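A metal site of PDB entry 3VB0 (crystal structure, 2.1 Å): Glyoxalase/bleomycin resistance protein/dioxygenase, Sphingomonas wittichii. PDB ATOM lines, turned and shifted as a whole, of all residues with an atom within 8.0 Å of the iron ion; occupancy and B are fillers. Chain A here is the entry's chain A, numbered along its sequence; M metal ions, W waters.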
ATOM      1  N   HIS A 147      -9.835 -13.547  -3.773  1.00  0.00           N
ATOM      2  CA  HIS A 147     -10.841 -13.436  -2.726  1.00  0.00           C
ATOM      3  C   HIS A 147     -11.951 -14.438  -2.826  1.00  0.00           C
ATOM      4  O   HIS A 147     -12.236 -14.965  -3.906  1.00  0.00           O
ATOM      5  CB  HIS A 147     -11.407 -12.008  -2.547  1.00  0.00           C
ATOM      6  CG  HIS A 147     -12.096 -11.442  -3.750  1.00  0.00           C
ATOM      7  ND1 HIS A 147     -11.545 -10.435  -4.506  1.00  0.00           N
ATOM      8  CD2 HIS A 147     -13.335 -11.664  -4.267  1.00  0.00           C
ATOM      9  CE1 HIS A 147     -12.383 -10.085  -5.468  1.00  0.00           C
ATOM     10  NE2 HIS A 147     -13.477 -10.816  -5.347  1.00  0.00           N
ATOM     11  N   LEU A 148     -12.525 -14.720  -1.669  1.00  0.00           N
ATOM     12  CA  LEU A 148     -13.665 -15.599  -1.536  1.00  0.00           C
ATOM     13  C   LEU A 148     -14.806 -14.795  -0.925  1.00  0.00           C
ATOM     14  O   LEU A 148     -14.604 -14.124   0.099  1.00  0.00           O
ATOM     15  CB  LEU A 148     -13.303 -16.768  -0.619  1.00  0.00           C
ATOM     16  CG  LEU A 148     -14.308 -17.900  -0.403  1.00  0.00           C
ATOM     17  CD1 LEU A 148     -14.391 -18.712  -1.666  1.00  0.00           C
ATOM     18  CD2 LEU A 148     -13.817 -18.762   0.746  1.00  0.00           C
ATOM     19  N   VAL A 149     -15.993 -14.885  -1.515  1.00  0.00           N
ATOM     20  CA  VAL A 149     -17.174 -14.236  -0.973  1.00  0.00           C
ATOM     21  C   VAL A 149     -18.146 -15.334  -0.519  1.00  0.00           C
ATOM     22  O   VAL A 149     -18.493 -16.234  -1.304  1.00  0.00           O
ATOM     23  CB  VAL A 149     -17.823 -13.276  -2.032  1.00  0.00           C
ATOM     24  CG1 VAL A 149     -19.056 -12.590  -1.482  1.00  0.00           C
ATOM     25  CG2 VAL A 149     -16.815 -12.224  -2.505  1.00  0.00           C
ATOM     26  N   PHE A 183     -16.798  -6.029   2.841  1.00  0.00           N
ATOM     27  CA  PHE A 183     -15.537  -6.453   2.236  1.00  0.00           C
ATOM     28  C   PHE A 183     -14.389  -6.267   3.197  1.00  0.00           C
ATOM     29  O   PHE A 183     -14.199  -5.158   3.733  1.00  0.00           O
ATOM     30  CB  PHE A 183     -15.293  -5.659   0.953  1.00  0.00           C
ATOM     31  CG  PHE A 183     -16.393  -5.801  -0.063  1.00  0.00           C
ATOM     32  CD1 PHE A 183     -16.232  -6.644  -1.154  1.00  0.00           C
ATOM     33  CD2 PHE A 183     -17.592  -5.108   0.075  1.00  0.00           C
ATOM     34  CE1 PHE A 183     -17.229  -6.786  -2.093  1.00  0.00           C
ATOM     35  CE2 PHE A 183     -18.600  -5.225  -0.851  1.00  0.00           C
ATOM     36  CZ  PHE A 183     -18.426  -6.051  -1.941  1.00  0.00           C
ATOM     37  N   HIS A 191      -9.833  -6.829  -0.941  1.00  0.00           N
ATOM     38  CA  HIS A 191     -10.458  -7.752  -0.022  1.00  0.00           C
ATOM     39  C   HIS A 191     -10.044  -9.177  -0.324  1.00  0.00           C
ATOM     40  O   HIS A 191      -9.850  -9.526  -1.476  1.00  0.00           O
ATOM     41  CB  HIS A 191     -11.974  -7.599   0.042  1.00  0.00           C
ATOM     42  CG  HIS A 191     -12.693  -7.865  -1.249  1.00  0.00           C
ATOM     43  ND1 HIS A 191     -12.764  -6.928  -2.264  1.00  0.00           N
ATOM     44  CD2 HIS A 191     -13.463  -8.901  -1.652  1.00  0.00           C
ATOM     45  CE1 HIS A 191     -13.510  -7.389  -3.245  1.00  0.00           C
ATOM     46  NE2 HIS A 191     -13.956  -8.593  -2.905  1.00  0.00           N
ATOM     47  N   ALA A 194     -15.308 -11.473   1.487  1.00  0.00           N
ATOM     48  CA  ALA A 194     -16.497 -10.618   1.646  1.00  0.00           C
ATOM     49  C   ALA A 194     -17.649 -11.428   2.214  1.00  0.00           C
ATOM     50  O   ALA A 194     -17.797 -12.602   1.900  1.00  0.00           O
ATOM     51  CB  ALA A 194     -16.914  -9.967   0.329  1.00  0.00           C
ATOM     52  N   HIS A 208     -20.558 -17.523  -2.636  1.00  0.00           N
ATOM     53  CA  HIS A 208     -21.097 -16.648  -3.677  1.00  0.00           C
ATOM     54  C   HIS A 208     -20.182 -16.677  -4.908  1.00  0.00           C
ATOM     55  O   HIS A 208     -20.614 -17.033  -6.010  1.00  0.00           O
ATOM     56  CB  HIS A 208     -21.246 -15.215  -3.178  1.00  0.00           C
ATOM     57  CG  HIS A 208     -21.766 -14.298  -4.219  1.00  0.00           C
ATOM     58  ND1 HIS A 208     -20.949 -13.516  -5.014  1.00  0.00           N
ATOM     59  CD2 HIS A 208     -23.035 -14.099  -4.679  1.00  0.00           C
ATOM     60  CE1 HIS A 208     -21.683 -12.843  -5.880  1.00  0.00           C
ATOM     61  NE2 HIS A 208     -22.950 -13.178  -5.701  1.00  0.00           N
ATOM     62  N   HIS A 209     -18.932 -16.271  -4.713  1.00  0.00           N
ATOM     63  CA  HIS A 209     -17.936 -16.414  -5.763  1.00  0.00           C
ATOM     64  C   HIS A 209     -16.529 -16.473  -5.212  1.00  0.00           C
ATOM     65  O   HIS A 209     -16.276 -16.163  -4.041  1.00  0.00           O
ATOM     66  CB  HIS A 209     -18.024 -15.314  -6.841  1.00  0.00           C
ATOM     67  CG  HIS A 209     -17.504 -13.970  -6.423  1.00  0.00           C
ATOM     68  ND1 HIS A 209     -18.293 -13.049  -5.770  1.00  0.00           N
ATOM     69  CD2 HIS A 209     -16.307 -13.370  -6.614  1.00  0.00           C
ATOM     70  CE1 HIS A 209     -17.593 -11.945  -5.569  1.00  0.00           C
ATOM     71  NE2 HIS A 209     -16.383 -12.112  -6.062  1.00  0.00           N
ATOM     72  N   LEU A 210     -15.634 -16.823  -6.122  1.00  0.00           N
ATOM     73  CA  LEU A 210     -14.205 -16.836  -5.930  1.00  0.00           C
ATOM     74  C   LEU A 210     -13.641 -15.893  -6.980  1.00  0.00           C
ATOM     75  O   LEU A 210     -14.156 -15.843  -8.103  1.00  0.00           O
ATOM     76  CB  LEU A 210     -13.709 -18.264  -6.215  1.00  0.00           C
ATOM     77  CG  LEU A 210     -12.231 -18.517  -6.400  1.00  0.00           C
ATOM     78  CD1 LEU A 210     -11.515 -18.013  -5.118  1.00  0.00           C
ATOM     79  CD2 LEU A 210     -12.057 -20.019  -6.546  1.00  0.00           C
ATOM     80  N   MET A 211     -12.559 -15.191  -6.650  1.00  0.00           N
ATOM     81  CA  MET A 211     -11.931 -14.329  -7.644  1.00  0.00           C
ATOM     82  C   MET A 211     -10.450 -14.591  -7.772  1.00  0.00           C
ATOM     83  O   MET A 211      -9.738 -14.694  -6.763  1.00  0.00           O
ATOM     84  CB  MET A 211     -12.185 -12.855  -7.291  1.00  0.00           C
ATOM     85  CG  MET A 211     -11.579 -11.813  -8.242  1.00  0.00           C
ATOM     86  SD  MET A 211      -9.882 -11.337  -7.842  1.00  0.00           S
ATOM     87  CE  MET A 211      -9.696  -9.979  -9.002  1.00  0.00           C
ATOM     88  N   LEU A 212      -9.970 -14.684  -9.013  1.00  0.00           N
ATOM     89  CA  LEU A 212      -8.542 -14.700  -9.312  1.00  0.00           C
ATOM     90  C   LEU A 212      -8.176 -13.428 -10.081  1.00  0.00           C
ATOM     91  O   LEU A 212      -9.024 -12.835 -10.750  1.00  0.00           O
ATOM     92  CB  LEU A 212      -8.161 -15.940 -10.134  1.00  0.00           C
ATOM     93  CG  LEU A 212      -8.571 -17.279  -9.514  1.00  0.00           C
ATOM     94  CD1 LEU A 212      -8.213 -18.423 -10.411  1.00  0.00           C
ATOM     95  CD2 LEU A 212      -7.978 -17.455  -8.099  1.00  0.00           C
ATOM     96  N   HIS A 241     -15.921  -2.757 -10.719  1.00  0.00           N
ATOM     97  CA  HIS A 241     -16.579  -2.610  -9.425  1.00  0.00           C
ATOM     98  C   HIS A 241     -16.255  -1.253  -8.824  1.00  0.00           C
ATOM     99  O   HIS A 241     -15.176  -0.713  -9.024  1.00  0.00           O
ATOM    100  CB  HIS A 241     -16.196  -3.729  -8.458  1.00  0.00           C
ATOM    101  CG  HIS A 241     -16.926  -5.013  -8.697  1.00  0.00           C
ATOM    102  ND1 HIS A 241     -18.305  -5.096  -8.730  1.00  0.00           N
ATOM    103  CD2 HIS A 241     -16.475  -6.275  -8.894  1.00  0.00           C
ATOM    104  CE1 HIS A 241     -18.663  -6.349  -8.954  1.00  0.00           C
ATOM    105  NE2 HIS A 241     -17.569  -7.084  -9.054  1.00  0.00           N
ATOM    106  N   ASN A 243     -16.061  -0.434  -5.553  1.00  0.00           N
ATOM    107  CA  ASN A 243     -15.170  -0.455  -4.392  1.00  0.00           C
ATOM    108  C   ASN A 243     -13.739  -0.867  -4.721  1.00  0.00           C
ATOM    109  O   ASN A 243     -12.812  -0.085  -4.491  1.00  0.00           O
ATOM    110  CB  ASN A 243     -15.755  -1.230  -3.196  1.00  0.00           C
ATOM    111  CG  ASN A 243     -16.133  -2.656  -3.520  1.00  0.00           C
ATOM    112  OD1 ASN A 243     -16.349  -3.032  -4.681  1.00  0.00           O
ATOM    113  ND2 ASN A 243     -16.246  -3.474  -2.492  1.00  0.00           N
ATOM    114  N   ASP A 244     -13.552  -2.067  -5.256  1.00  0.00           N
ATOM    115  CA  ASP A 244     -12.194  -2.533  -5.556  1.00  0.00           C
ATOM    116  C   ASP A 244     -11.620  -2.068  -6.914  1.00  0.00           C
ATOM    117  O   ASP A 244     -10.424  -2.250  -7.174  1.00  0.00           O
ATOM    118  CB  ASP A 244     -12.021  -4.058  -5.314  1.00  0.00           C
ATOM    119  CG  ASP A 244     -12.857  -4.907  -6.252  1.00  0.00           C
ATOM    120  OD1 ASP A 244     -13.563  -4.353  -7.117  1.00  0.00           O
ATOM    121  OD2 ASP A 244     -12.793  -6.159  -6.132  1.00  0.00           O
ATOM    122  N   VAL A 246     -11.836  -3.231  -9.696  1.00  0.00           N
ATOM    123  CA  VAL A 246     -11.455  -4.366 -10.520  1.00  0.00           C
ATOM    124  C   VAL A 246     -12.170  -4.353 -11.873  1.00  0.00           C
ATOM    125  O   VAL A 246     -13.382  -4.153 -11.954  1.00  0.00           O
ATOM    126  CB  VAL A 246     -11.717  -5.701  -9.741  1.00  0.00           C
ATOM    127  CG1 VAL A 246     -11.931  -6.839 -10.660  1.00  0.00           C
ATOM    128  CG2 VAL A 246     -10.556  -5.998  -8.842  1.00  0.00           C
ATOM    129  N   SER A 248     -13.388  -6.782 -14.432  1.00  0.00           N
ATOM    130  CA  SER A 248     -13.624  -8.224 -14.362  1.00  0.00           C
ATOM    131  C   SER A 248     -14.900  -8.671 -15.050  1.00  0.00           C
ATOM    132  O   SER A 248     -15.743  -7.851 -15.390  1.00  0.00           O
ATOM    133  CB  SER A 248     -13.706  -8.686 -12.904  1.00  0.00           C
ATOM    134  OG  SER A 248     -14.917  -8.248 -12.303  1.00  0.00           O
ATOM    135  N   PHE A 249     -15.012  -9.990 -15.239  1.00  0.00           N
ATOM    136  CA  PHE A 249     -16.278 -10.620 -15.583  1.00  0.00           C
ATOM    137  C   PHE A 249     -16.518 -11.811 -14.655  1.00  0.00           C
ATOM    138  O   PHE A 249     -15.595 -12.256 -13.959  1.00  0.00           O
ATOM    139  CB  PHE A 249     -16.282 -11.081 -17.035  1.00  0.00           C
ATOM    140  CG  PHE A 249     -15.376 -12.247 -17.296  1.00  0.00           C
ATOM    141  CD1 PHE A 249     -15.880 -13.541 -17.293  1.00  0.00           C
ATOM    142  CD2 PHE A 249     -14.026 -12.034 -17.541  1.00  0.00           C
ATOM    143  CE1 PHE A 249     -15.041 -14.633 -17.531  1.00  0.00           C
ATOM    144  CE2 PHE A 249     -13.179 -13.110 -17.769  1.00  0.00           C
ATOM    145  CZ  PHE A 249     -13.699 -14.409 -17.765  1.00  0.00           C
ATOM    146  N   TYR A 250     -17.747 -12.316 -14.638  1.00  0.00           N
ATOM    147  CA  TYR A 250     -18.113 -13.463 -13.819  1.00  0.00           C
ATOM    148  C   TYR A 250     -18.687 -14.567 -14.678  1.00  0.00           C
ATOM    149  O   TYR A 250     -19.376 -14.304 -15.673  1.00  0.00           O
ATOM    150  CB  TYR A 250     -19.186 -13.079 -12.779  1.00  0.00           C
ATOM    151  CG  TYR A 250     -18.738 -12.214 -11.639  1.00  0.00           C
ATOM    152  CD1 TYR A 250     -18.735 -12.707 -10.333  1.00  0.00           C
ATOM    153  CD2 TYR A 250     -18.356 -10.887 -11.845  1.00  0.00           C
ATOM    154  CE1 TYR A 250     -18.366 -11.889  -9.259  1.00  0.00           C
ATOM    155  CE2 TYR A 250     -17.969 -10.064 -10.772  1.00  0.00           C
ATOM    156  CZ  TYR A 250     -17.995 -10.569  -9.485  1.00  0.00           C
ATOM    157  OH  TYR A 250     -17.589  -9.776  -8.423  1.00  0.00           O
ATOM    158  N   VAL A 259     -17.203 -17.812 -10.674  1.00  0.00           N
ATOM    159  CA  VAL A 259     -15.774 -17.563 -10.704  1.00  0.00           C
ATOM    160  C   VAL A 259     -15.559 -16.236 -11.428  1.00  0.00           C
ATOM    161  O   VAL A 259     -16.134 -16.014 -12.481  1.00  0.00           O
ATOM    162  CB  VAL A 259     -15.000 -18.697 -11.396  1.00  0.00           C
ATOM    163  CG1 VAL A 259     -13.552 -18.274 -11.630  1.00  0.00           C
ATOM    164  CG2 VAL A 259     -15.045 -19.969 -10.557  1.00  0.00           C
ATOM    165  N   GLU A 260     -14.748 -15.380 -10.827  1.00  0.00           N
ATOM    166  CA  GLU A 260     -14.479 -14.042 -11.356  1.00  0.00           C
ATOM    167  C   GLU A 260     -13.008 -13.959 -11.731  1.00  0.00           C
ATOM    168  O   GLU A 260     -12.140 -14.400 -10.969  1.00  0.00           O
ATOM    169  CB  GLU A 260     -14.827 -12.982 -10.306  1.00  0.00           C
ATOM    170  CG  GLU A 260     -14.589 -11.511 -10.751  1.00  0.00           C
ATOM    171  CD  GLU A 260     -14.602 -10.501  -9.580  1.00  0.00           C
ATOM    172  OE1 GLU A 260     -14.713 -10.937  -8.396  1.00  0.00           O
ATOM    173  OE2 GLU A 260     -14.483  -9.269  -9.857  1.00  0.00           O
ATOM    174  N   LEU A 261     -12.723 -13.439 -12.915  1.00  0.00           N
ATOM    175  CA  LEU A 261     -11.342 -13.139 -13.269  1.00  0.00           C
ATOM    176  C   LEU A 261     -11.260 -11.648 -13.473  1.00  0.00           C
ATOM    177  O   LEU A 261     -11.983 -11.099 -14.290  1.00  0.00           O
ATOM    178  CB  LEU A 261     -10.879 -13.895 -14.527  1.00  0.00           C
ATOM    179  CG  LEU A 261      -9.406 -13.654 -14.910  1.00  0.00           C
ATOM    180  CD1 LEU A 261      -8.456 -14.365 -13.922  1.00  0.00           C
ATOM    181  CD2 LEU A 261      -9.129 -14.135 -16.329  1.00  0.00           C
ATOM    182  N   GLY A 262     -10.362 -11.001 -12.729  1.00  0.00           N
ATOM    183  CA  GLY A 262     -10.284  -9.540 -12.770  1.00  0.00           C
ATOM    184  C   GLY A 262      -8.886  -8.986 -12.942  1.00  0.00           C
ATOM    185  O   GLY A 262      -7.899  -9.723 -12.852  1.00  0.00           O
ATOM    186  N   HIS A 287     -20.748  -5.066 -16.094  1.00  0.00           N
ATOM    187  CA  HIS A 287     -21.207  -6.066 -15.113  1.00  0.00           C
ATOM    188  C   HIS A 287     -22.702  -6.339 -15.218  1.00  0.00           C
ATOM    189  O   HIS A 287     -23.408  -6.423 -14.207  1.00  0.00           O
ATOM    190  CB  HIS A 287     -20.849  -5.647 -13.680  1.00  0.00           C
ATOM    191  CG  HIS A 287     -19.425  -5.914 -13.313  1.00  0.00           C
ATOM    192  ND1 HIS A 287     -18.766  -5.177 -12.349  1.00  0.00           N
ATOM    193  CD2 HIS A 287     -18.534  -6.827 -13.771  1.00  0.00           C
ATOM    194  CE1 HIS A 287     -17.527  -5.627 -12.240  1.00  0.00           C
ATOM    195  NE2 HIS A 287     -17.357  -6.623 -13.082  1.00  0.00           N
HETATM  196 FE    FE M   1     -15.223 -10.296  -6.511  1.00  0.00          FE
HETATM  197  O   HOH W   1     -14.242  -8.372  -7.215  1.00  0.00           O
HETATM  198  O   HOH W   2     -16.001  -9.189  -4.861  1.00  0.00           O
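Water W1 lies within hydrogen-bond range of the side-chain carboxylate of Glu 260 (2.8 Å) and the side-chain carboxylate of Asp 244 (2.9 Å).
Residues that only touch the iron ion: Tyr 250 (3.1 Å).
Four residues have an atom within 4 Å of the iron ion: His 147, His 209, Tyr 250 and Glu 260.
The nearest printed residue that does not touch the iron ion is Met 211 (4.05 Å).
The iron ion is bound by OE1 of Glu 260 (2.1 Å), water W2 (2.1 Å), NE2 of His 147 (2.2 Å), NE2 of His 209 (2.2 Å) and water W1 (2.3 Å).
The iron ion has five donor atoms within binding distance.
The backbone NH of Glu 260 sits at hydrogen-bond distance from the backbone carbonyl oxygen of Leu 210, at 2.8 Å.
A ring nitrogen (ND1) of His 209 lies within hydrogen-bond range of a ring nitrogen (ND1) of His 208 (2.8 Å).
The backbone NH (N) of Val 149 lies within hydrogen-bond range of the backbone carbonyl oxygen (O) of His 209, at 2.8 Å.
ND1 of His 147 sits close to NE2 of His 191 (3.4 Å).
OH of Tyr 250 sits at hydrogen-bond distance from NE2 of His 241 (2.8 Å).
The backbone carbonyl oxygen (O) of His 147 sits at hydrogen-bond distance from the backbone NH (N) of Met 211.
OE2 of Glu 260 is in hydrogen-bond range of OG of Ser 248 (2.7 Å).
O of Glu 260 sits at hydrogen-bond distance from N of Leu 212 (2.9 Å).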
